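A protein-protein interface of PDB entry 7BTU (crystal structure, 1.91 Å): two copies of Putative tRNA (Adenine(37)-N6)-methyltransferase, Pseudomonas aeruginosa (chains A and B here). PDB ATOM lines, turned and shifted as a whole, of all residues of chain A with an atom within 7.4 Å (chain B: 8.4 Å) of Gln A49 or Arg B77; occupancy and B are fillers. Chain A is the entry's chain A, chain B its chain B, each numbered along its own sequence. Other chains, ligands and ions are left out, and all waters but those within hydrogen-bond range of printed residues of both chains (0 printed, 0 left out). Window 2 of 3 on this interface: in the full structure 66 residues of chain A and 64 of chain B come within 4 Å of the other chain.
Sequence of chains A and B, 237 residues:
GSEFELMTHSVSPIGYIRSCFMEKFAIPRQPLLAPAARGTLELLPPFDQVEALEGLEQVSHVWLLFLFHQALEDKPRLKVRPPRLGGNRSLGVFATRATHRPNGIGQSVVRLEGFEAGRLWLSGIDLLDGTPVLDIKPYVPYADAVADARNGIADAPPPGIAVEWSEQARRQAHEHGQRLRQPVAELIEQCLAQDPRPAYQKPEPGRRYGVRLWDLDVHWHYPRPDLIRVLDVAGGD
N of Gly B92 sits at hydrogen-bond distance from O of Glu A54, at 2.8 Å. The backbone carbonyl oxygen (O) of Ala A52 sits at hydrogen-bond distance from the backbone NH (N) of Val B93, 3.4 Å away. The backbone carbonyl oxygen (O) of Ala A52 sits at hydrogen-bond distance from the backbone NH (N) of Phe B94 (3.1 Å). The side-chain amide oxygen of Gln A49 is in hydrogen-bond range of the guanidinium group of Arg B77 (2.7 Å).
The backbone carbonyl oxygen (O) of Val B93 sits at hydrogen-bond distance from the guanidinium group (NH2) of Arg B101 (3.2 Å). The backbone NH (N) of Lys B79 is in hydrogen-bond range of the backbone carbonyl oxygen (O) of Leu B91 (2.7 Å). O of Val B93 lies within hydrogen-bond range of OG1 of Thr B96. The backbone carbonyl oxygen of Arg B77 lies within hydrogen-bond range of the backbone NH of Val B93.
Pro A46 touches Arg B77. Phe A47 touches Pro B102 (CE1 to CG, 3.5 Å). Arg B77 touches Glu A51. Glu A51 touches Gly B92 (O to CA, 3.1 Å). O of Arg B77 touches CA of Ala A52, 3.5 Å away. Ala A52 touches Gly B92. Leu A53 touches Phe B94 (CD2 to CD2, 3.8 Å). O of Glu A54 touches CA of Leu B91 (3.6 Å). O of Glu A54 touches CB of Ala B95, 3.2 Å away.
Of chain B, only Arg B77 comes within 4 Å of Gln A49. Of chain B, only Arg B77, Gly B92, Val B93 and Phe B94 come within 4 Å of Ala A52. Printed residues of chain A within 4 Å of Phe B94: Ala A52 (3.1 Å) and Leu A53 (3.8 Å). Printed residues of chain B within 4 Å of Pro A46: Arg B77. Of the printed residues of chain B, Phe A47 touches Pro B102. Val B80 touches none of the printed residues of chain A. Gly A118 touches none of the printed residues of chain B. The nearest residue of chain B that does not touch Gln A49 is Phe B94 (6.5 Å).
Of the 16 printed residues of chain B, 7 touch a printed residue of chain A. Printed residues of chain B that touch a printed residue of chain A: Arg B77, Leu B91, Gly B92, Val B93, Phe B94, Ala B95 and Pro B102. Hydrophobic or aromatic side chains of chain B within 4 Å of the printed part of chain A: Leu B91, Phe B94, Ala B95 and Pro B102. Among the printed residues, 13 pairs touch across the chains.
No position is printed for both chains. Of the 13 pairs that touch across the chains among the printed residues, none has its exchanged pair printed and touching as well.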
ATOM      1  N   LEU A  43      18.096  -6.689  16.349  1.00  0.00           N
ATOM      2  CA  LEU A  43      17.869  -6.350  17.746  1.00  0.00           C
ATOM      3  C   LEU A  43      16.425  -5.975  17.971  1.00  0.00           C
ATOM      4  O   LEU A  43      15.808  -5.345  17.126  1.00  0.00           O
ATOM      5  CB  LEU A  43      18.774  -5.178  18.195  1.00  0.00           C
ATOM      6  CG  LEU A  43      20.242  -5.575  18.115  1.00  0.00           C
ATOM      7  CD1 LEU A  43      21.132  -4.339  18.139  1.00  0.00           C
ATOM      8  CD2 LEU A  43      20.636  -6.601  19.218  1.00  0.00           C
ATOM      9  N   LEU A  44      15.884  -6.353  19.167  1.00  0.00           N
ATOM     10  CA  LEU A  44      14.544  -6.068  19.676  1.00  0.00           C
ATOM     11  C   LEU A  44      14.579  -4.813  20.538  1.00  0.00           C
ATOM     12  O   LEU A  44      15.580  -4.566  21.227  1.00  0.00           O
ATOM     13  CB  LEU A  44      14.080  -7.220  20.553  1.00  0.00           C
ATOM     14  CG  LEU A  44      14.174  -8.549  19.856  1.00  0.00           C
ATOM     15  CD1 LEU A  44      13.966  -9.697  20.865  1.00  0.00           C
ATOM     16  CD2 LEU A  44      13.135  -8.492  18.757  1.00  0.00           C
ATOM     17  N   PRO A  45      13.501  -4.025  20.567  1.00  0.00           N
ATOM     18  CA  PRO A  45      13.444  -2.920  21.509  1.00  0.00           C
ATOM     19  C   PRO A  45      13.494  -3.430  22.933  1.00  0.00           C
ATOM     20  O   PRO A  45      12.970  -4.517  23.243  1.00  0.00           O
ATOM     21  CB  PRO A  45      12.102  -2.236  21.186  1.00  0.00           C
ATOM     22  CG  PRO A  45      11.328  -3.233  20.366  1.00  0.00           C
ATOM     23  CD  PRO A  45      12.282  -4.173  19.750  1.00  0.00           C
ATOM     24  N   PRO A  46      14.128  -2.672  23.846  1.00  0.00           N
ATOM     25  CA  PRO A  46      14.709  -1.336  23.593  1.00  0.00           C
ATOM     26  C   PRO A  46      16.175  -1.404  23.101  1.00  0.00           C
ATOM     27  O   PRO A  46      16.894  -0.381  23.010  1.00  0.00           O
ATOM     28  CB  PRO A  46      14.632  -0.678  24.972  1.00  0.00           C
ATOM     29  CG  PRO A  46      14.918  -1.846  25.931  1.00  0.00           C
ATOM     30  CD  PRO A  46      14.257  -3.069  25.269  1.00  0.00           C
ATOM     31  N   PHE A  47      16.618  -2.611  22.755  1.00  0.00           N
ATOM     32  CA  PHE A  47      18.039  -2.817  22.440  1.00  0.00           C
ATOM     33  C   PHE A  47      18.340  -2.456  21.000  1.00  0.00           C
ATOM     34  O   PHE A  47      19.510  -2.468  20.595  1.00  0.00           O
ATOM     35  CB  PHE A  47      18.451  -4.283  22.701  1.00  0.00           C
ATOM     36  CG  PHE A  47      17.981  -4.797  24.039  1.00  0.00           C
ATOM     37  CD1 PHE A  47      18.510  -4.281  25.209  1.00  0.00           C
ATOM     38  CD2 PHE A  47      16.933  -5.727  24.121  1.00  0.00           C
ATOM     39  CE1 PHE A  47      18.054  -4.696  26.465  1.00  0.00           C
ATOM     40  CE2 PHE A  47      16.484  -6.166  25.368  1.00  0.00           C
ATOM     41  CZ  PHE A  47      17.037  -5.635  26.540  1.00  0.00           C
ATOM     42  N   ASP A  48      17.321  -2.010  20.266  1.00  0.00           N
ATOM     43  CA  ASP A  48      17.476  -1.590  18.885  1.00  0.00           C
ATOM     44  C   ASP A  48      17.744  -0.095  18.798  1.00  0.00           C
ATOM     45  O   ASP A  48      17.825   0.463  17.704  1.00  0.00           O
ATOM     46  CB  ASP A  48      16.217  -1.943  18.085  1.00  0.00           C
ATOM     47  CG  ASP A  48      14.934  -1.319  18.686  1.00  0.00           C
ATOM     48  OD1 ASP A  48      14.976  -0.781  19.807  1.00  0.00           O
ATOM     49  OD2 ASP A  48      13.868  -1.381  18.036  1.00  0.00           O
ATOM     50  N   GLN A  49      17.915   0.564  19.925  1.00  0.00           N
ATOM     51  CA  GLN A  49      18.141   1.995  19.864  1.00  0.00           C
ATOM     52  C   GLN A  49      19.628   2.211  19.566  1.00  0.00           C
ATOM     53  O   GLN A  49      20.477   1.518  20.117  1.00  0.00           O
ATOM     54  CB  GLN A  49      17.703   2.668  21.189  1.00  0.00           C
ATOM     55  CG  GLN A  49      16.175   2.564  21.506  1.00  0.00           C
ATOM     56  CD  GLN A  49      15.803   2.825  22.996  1.00  0.00           C
ATOM     57  OE1 GLN A  49      16.592   3.376  23.761  1.00  0.00           O
ATOM     58  NE2 GLN A  49      14.605   2.413  23.394  1.00  0.00           N
ATOM     59  N   VAL A  50      19.938   3.221  18.744  1.00  0.00           N
ATOM     60  CA  VAL A  50      21.314   3.392  18.257  1.00  0.00           C
ATOM     61  C   VAL A  50      22.273   3.754  19.400  1.00  0.00           C
ATOM     62  O   VAL A  50      23.462   3.431  19.335  1.00  0.00           O
ATOM     63  CB  VAL A  50      21.342   4.444  17.101  1.00  0.00           C
ATOM     64  CG1 VAL A  50      20.965   5.824  17.581  1.00  0.00           C
ATOM     65  CG2 VAL A  50      22.705   4.524  16.435  1.00  0.00           C
ATOM     66  N   GLU A  51      21.764   4.337  20.488  1.00  0.00           N
ATOM     67  CA  GLU A  51      22.633   4.690  21.611  1.00  0.00           C
ATOM     68  C   GLU A  51      23.278   3.451  22.230  1.00  0.00           C
ATOM     69  O   GLU A  51      24.357   3.544  22.822  1.00  0.00           O
ATOM     70  CB  GLU A  51      21.838   5.419  22.680  1.00  0.00           C
ATOM     71  CG  GLU A  51      21.446   6.829  22.348  1.00  0.00           C
ATOM     72  CD  GLU A  51      20.213   6.920  21.449  1.00  0.00           C
ATOM     73  OE1 GLU A  51      19.542   5.886  21.227  1.00  0.00           O
ATOM     74  OE2 GLU A  51      19.907   8.046  20.981  1.00  0.00           O
ATOM     75  N   ALA A  52      22.643   2.282  22.105  1.00  0.00           N
ATOM     76  CA  ALA A  52      23.216   1.092  22.733  1.00  0.00           C
ATOM     77  C   ALA A  52      24.506   0.625  22.069  1.00  0.00           C
ATOM     78  O   ALA A  52      25.238  -0.171  22.673  1.00  0.00           O
ATOM     79  CB  ALA A  52      22.200  -0.044  22.747  1.00  0.00           C
ATOM     80  N   LEU A  53      24.809   1.128  20.868  1.00  0.00           N
ATOM     81  CA  LEU A  53      25.912   0.659  20.047  1.00  0.00           C
ATOM     82  C   LEU A  53      27.036   1.662  19.917  1.00  0.00           C
ATOM     83  O   LEU A  53      28.034   1.349  19.256  1.00  0.00           O
ATOM     84  CB  LEU A  53      25.414   0.311  18.639  1.00  0.00           C
ATOM     85  CG  LEU A  53      24.222  -0.643  18.721  1.00  0.00           C
ATOM     86  CD1 LEU A  53      23.660  -0.872  17.328  1.00  0.00           C
ATOM     87  CD2 LEU A  53      24.643  -1.975  19.345  1.00  0.00           C
ATOM     88  N   GLU A  54      26.869   2.858  20.493  1.00  0.00           N
ATOM     89  CA  GLU A  54      27.783   3.973  20.294  1.00  0.00           C
ATOM     90  C   GLU A  54      29.190   3.586  20.718  1.00  0.00           C
ATOM     91  O   GLU A  54      29.418   3.187  21.860  1.00  0.00           O
ATOM     92  CB  GLU A  54      27.274   5.185  21.086  1.00  0.00           C
ATOM     93  N   GLU A 116      23.822  -0.374  12.230  1.00  0.00           N
ATOM     94  CA  GLU A 116      22.911   0.748  12.218  1.00  0.00           C
ATOM     95  C   GLU A 116      21.932   0.483  13.344  1.00  0.00           C
ATOM     96  O   GLU A 116      21.987  -0.568  13.990  1.00  0.00           O
ATOM     97  CB  GLU A 116      22.198   0.858  10.878  1.00  0.00           C
ATOM     98  CG  GLU A 116      21.357  -0.366  10.570  1.00  0.00           C
ATOM     99  CD  GLU A 116      20.618  -0.210   9.274  1.00  0.00           C
ATOM    100  OE1 GLU A 116      21.031   0.656   8.482  1.00  0.00           O
ATOM    101  OE2 GLU A 116      19.614  -0.917   9.055  1.00  0.00           O
ATOM    102  N   ALA A 117      21.016   1.414  13.558  1.00  0.00           N
ATOM    103  CA  ALA A 117      19.961   1.193  14.535  1.00  0.00           C
ATOM    104  C   ALA A 117      19.285  -0.164  14.317  1.00  0.00           C
ATOM    105  O   ALA A 117      18.725  -0.446  13.254  1.00  0.00           O
ATOM    106  CB  ALA A 117      18.935   2.334  14.458  1.00  0.00           C
ATOM    107  N   GLY A 118      19.345  -1.011  15.333  1.00  0.00           N
ATOM    108  CA  GLY A 118      18.618  -2.260  15.295  1.00  0.00           C
ATOM    109  C   GLY A 118      19.262  -3.392  14.526  1.00  0.00           C
ATOM    110  O   GLY A 118      18.645  -4.464  14.421  1.00  0.00           O
ATOM    111  N   LYS B  75      16.679  -0.873  32.571  1.00  0.00           N
ATOM    112  CA  LYS B  75      17.291  -1.174  31.272  1.00  0.00           C
ATOM    113  C   LYS B  75      18.420  -0.179  30.956  1.00  0.00           C
ATOM    114  O   LYS B  75      18.156   0.927  30.476  1.00  0.00           O
ATOM    115  CB  LYS B  75      16.221  -1.158  30.158  1.00  0.00           C
ATOM    116  N   PRO B  76      19.667  -0.577  31.223  1.00  0.00           N
ATOM    117  CA  PRO B  76      20.836   0.292  31.042  1.00  0.00           C
ATOM    118  C   PRO B  76      21.447   0.063  29.657  1.00  0.00           C
ATOM    119  O   PRO B  76      21.969  -1.026  29.381  1.00  0.00           O
ATOM    120  CB  PRO B  76      21.872   0.024  32.134  1.00  0.00           C
ATOM    121  N   ARG B  77      21.395   1.098  28.794  1.00  0.00           N
ATOM    122  CA  ARG B  77      21.904   1.027  27.420  1.00  0.00           C
ATOM    123  C   ARG B  77      23.060   1.982  27.136  1.00  0.00           C
ATOM    124  O   ARG B  77      23.727   1.836  26.104  1.00  0.00           O
ATOM    125  CB  ARG B  77      20.788   1.332  26.399  1.00  0.00           C
ATOM    126  CG  ARG B  77      19.529   0.483  26.466  1.00  0.00           C
ATOM    127  CD  ARG B  77      18.354   1.268  25.810  1.00  0.00           C
ATOM    128  NE  ARG B  77      17.076   1.177  26.545  1.00  0.00           N
ATOM    129  CZ  ARG B  77      16.252   2.197  26.835  1.00  0.00           C
ATOM    130  NH1 ARG B  77      16.537   3.447  26.468  1.00  0.00           N
ATOM    131  NH2 ARG B  77      15.121   1.960  27.499  1.00  0.00           N
ATOM    132  N   LEU B  78      23.310   2.960  27.998  1.00  0.00           N
ATOM    133  CA  LEU B  78      24.353   3.946  27.763  1.00  0.00           C
ATOM    134  C   LEU B  78      25.219   4.051  29.010  1.00  0.00           C
ATOM    135  O   LEU B  78      24.706   4.048  30.129  1.00  0.00           O
ATOM    136  CB  LEU B  78      23.757   5.311  27.407  1.00  0.00           C
ATOM    137  N   LYS B  79      26.532   4.109  28.818  1.00  0.00           N
ATOM    138  CA  LYS B  79      27.482   4.207  29.924  1.00  0.00           C
ATOM    139  C   LYS B  79      28.171   5.563  29.823  1.00  0.00           C
ATOM    140  O   LYS B  79      28.730   5.898  28.772  1.00  0.00           O
ATOM    141  CB  LYS B  79      28.491   3.043  29.888  1.00  0.00           C
ATOM    142  N   VAL B  80      28.097   6.356  30.895  1.00  0.00           N
ATOM    143  CA  VAL B  80      28.659   7.711  30.885  1.00  0.00           C
ATOM    144  C   VAL B  80      29.863   7.830  31.819  1.00  0.00           C
ATOM    145  O   VAL B  80      30.580   6.854  32.050  1.00  0.00           O
ATOM    146  CB  VAL B  80      27.584   8.750  31.267  1.00  0.00           C
ATOM    147  N   SER B  90      29.710   9.480  26.133  1.00  0.00           N
ATOM    148  CA  SER B  90      29.014   8.264  26.580  1.00  0.00           C
ATOM    149  C   SER B  90      28.992   7.114  25.548  1.00  0.00           C
ATOM    150  O   SER B  90      28.561   7.284  24.378  1.00  0.00           O
ATOM    151  CB  SER B  90      27.574   8.617  26.991  1.00  0.00           C
ATOM    152  N   LEU B  91      29.376   5.917  25.990  1.00  0.00           N
ATOM    153  CA  LEU B  91      29.462   4.780  25.088  1.00  0.00           C
ATOM    154  C   LEU B  91      28.223   3.908  25.240  1.00  0.00           C
ATOM    155  O   LEU B  91      27.618   3.863  26.311  1.00  0.00           O
ATOM    156  CB  LEU B  91      30.708   3.937  25.387  1.00  0.00           C
ATOM    157  CG  LEU B  91      32.028   4.637  25.073  1.00  0.00           C
ATOM    158  CD1 LEU B  91      33.162   3.722  25.502  1.00  0.00           C
ATOM    159  CD2 LEU B  91      32.095   4.926  23.585  1.00  0.00           C
ATOM    160  N   GLY B  92      27.858   3.210  24.161  1.00  0.00           N
ATOM    161  CA  GLY B  92      26.806   2.222  24.255  1.00  0.00           C
ATOM    162  C   GLY B  92      27.199   1.042  25.124  1.00  0.00           C
ATOM    163  O   GLY B  92      28.360   0.630  25.176  1.00  0.00           O
ATOM    164  N   VAL B  93      26.218   0.482  25.827  1.00  0.00           N
ATOM    165  CA  VAL B  93      26.533  -0.630  26.723  1.00  0.00           C
ATOM    166  C   VAL B  93      27.178  -1.773  25.943  1.00  0.00           C
ATOM    167  O   VAL B  93      28.084  -2.452  26.447  1.00  0.00           O
ATOM    168  CB  VAL B  93      25.258  -1.097  27.474  1.00  0.00           C
ATOM    169  CG1 VAL B  93      24.238  -1.674  26.499  1.00  0.00           C
ATOM    170  CG2 VAL B  93      25.607  -2.160  28.574  1.00  0.00           C
ATOM    171  N   PHE B  94      26.771  -1.968  24.696  1.00  0.00           N
ATOM    172  CA  PHE B  94      27.308  -3.064  23.891  1.00  0.00           C
ATOM    173  C   PHE B  94      28.694  -2.754  23.342  1.00  0.00           C
ATOM    174  O   PHE B  94      29.313  -3.640  22.739  1.00  0.00           O
ATOM    175  CB  PHE B  94      26.338  -3.390  22.749  1.00  0.00           C
ATOM    176  CG  PHE B  94      25.018  -3.901  23.238  1.00  0.00           C
ATOM    177  CD1 PHE B  94      24.967  -4.890  24.205  1.00  0.00           C
ATOM    178  CD2 PHE B  94      23.823  -3.396  22.739  1.00  0.00           C
ATOM    179  CE1 PHE B  94      23.693  -5.407  24.648  1.00  0.00           C
ATOM    180  CE2 PHE B  94      22.597  -3.898  23.175  1.00  0.00           C
ATOM    181  CZ  PHE B  94      22.522  -4.873  24.138  1.00  0.00           C
ATOM    182  N   ALA B  95      29.172  -1.526  23.527  1.00  0.00           N
ATOM    183  CA  ALA B  95      30.539  -1.164  23.191  1.00  0.00           C
ATOM    184  C   ALA B  95      31.469  -1.286  24.400  1.00  0.00           C
ATOM    185  O   ALA B  95      32.639  -0.893  24.318  1.00  0.00           O
ATOM    186  CB  ALA B  95      30.570   0.275  22.645  1.00  0.00           C
ATOM    187  N   THR B  96      30.962  -1.810  25.515  1.00  0.00           N
ATOM    188  CA  THR B  96      31.675  -1.861  26.777  1.00  0.00           C
ATOM    189  C   THR B  96      31.534  -3.229  27.405  1.00  0.00           C
ATOM    190  O   THR B  96      30.666  -4.049  27.048  1.00  0.00           O
ATOM    191  CB  THR B  96      31.130  -0.853  27.813  1.00  0.00           C
ATOM    192  OG1 THR B  96      29.907  -1.387  28.355  1.00  0.00           O
ATOM    193  CG2 THR B  96      30.878   0.539  27.217  1.00  0.00           C
ATOM    194  N   HIS B 100      26.710  -3.548  34.540  1.00  0.00           N
ATOM    195  CA  HIS B 100      25.243  -3.455  34.530  1.00  0.00           C
ATOM    196  C   HIS B 100      24.854  -3.514  33.065  1.00  0.00           C
ATOM    197  O   HIS B 100      25.055  -2.548  32.334  1.00  0.00           O
ATOM    198  CB  HIS B 100      24.700  -2.174  35.173  1.00  0.00           C
ATOM    199  CG  HIS B 100      25.164  -1.939  36.581  1.00  0.00           C
ATOM    200  ND1 HIS B 100      26.380  -1.357  36.882  1.00  0.00           N
ATOM    201  CD2 HIS B 100      24.569  -2.203  37.772  1.00  0.00           C
ATOM    202  CE1 HIS B 100      26.513  -1.270  38.195  1.00  0.00           C
ATOM    203  NE2 HIS B 100      25.432  -1.785  38.758  1.00  0.00           N
ATOM    204  N   ARG B 101      24.365  -4.662  32.615  1.00  0.00           N
ATOM    205  CA  ARG B 101      24.069  -4.852  31.198  1.00  0.00           C
ATOM    206  C   ARG B 101      22.889  -5.813  31.025  1.00  0.00           C
ATOM    207  O   ARG B 101      22.517  -6.524  31.969  1.00  0.00           O
ATOM    208  CB  ARG B 101      25.310  -5.355  30.453  1.00  0.00           C
ATOM    209  CG  ARG B 101      25.784  -6.672  30.921  1.00  0.00           C
ATOM    210  CD  ARG B 101      27.179  -6.986  30.329  1.00  0.00           C
ATOM    211  NE  ARG B 101      27.283  -6.746  28.888  1.00  0.00           N
ATOM    212  CZ  ARG B 101      27.900  -5.701  28.322  1.00  0.00           C
ATOM    213  NH1 ARG B 101      28.453  -4.729  29.062  1.00  0.00           N
ATOM    214  NH2 ARG B 101      27.905  -5.599  27.009  1.00  0.00           N
ATOM    215  N   PRO B 102      22.226  -5.789  29.861  1.00  0.00           N
ATOM    216  CA  PRO B 102      21.097  -6.700  29.623  1.00  0.00           C
ATOM    217  C   PRO B 102      21.490  -8.136  29.930  1.00  0.00           C
ATOM    218  O   PRO B 102      22.566  -8.601  29.544  1.00  0.00           O
ATOM    219  CB  PRO B 102      20.795  -6.515  28.131  1.00  0.00           C
ATOM    220  CG  PRO B 102      21.269  -5.144  27.807  1.00  0.00           C
ATOM    221  CD  PRO B 102      22.446  -4.868  28.724  1.00  0.00           C
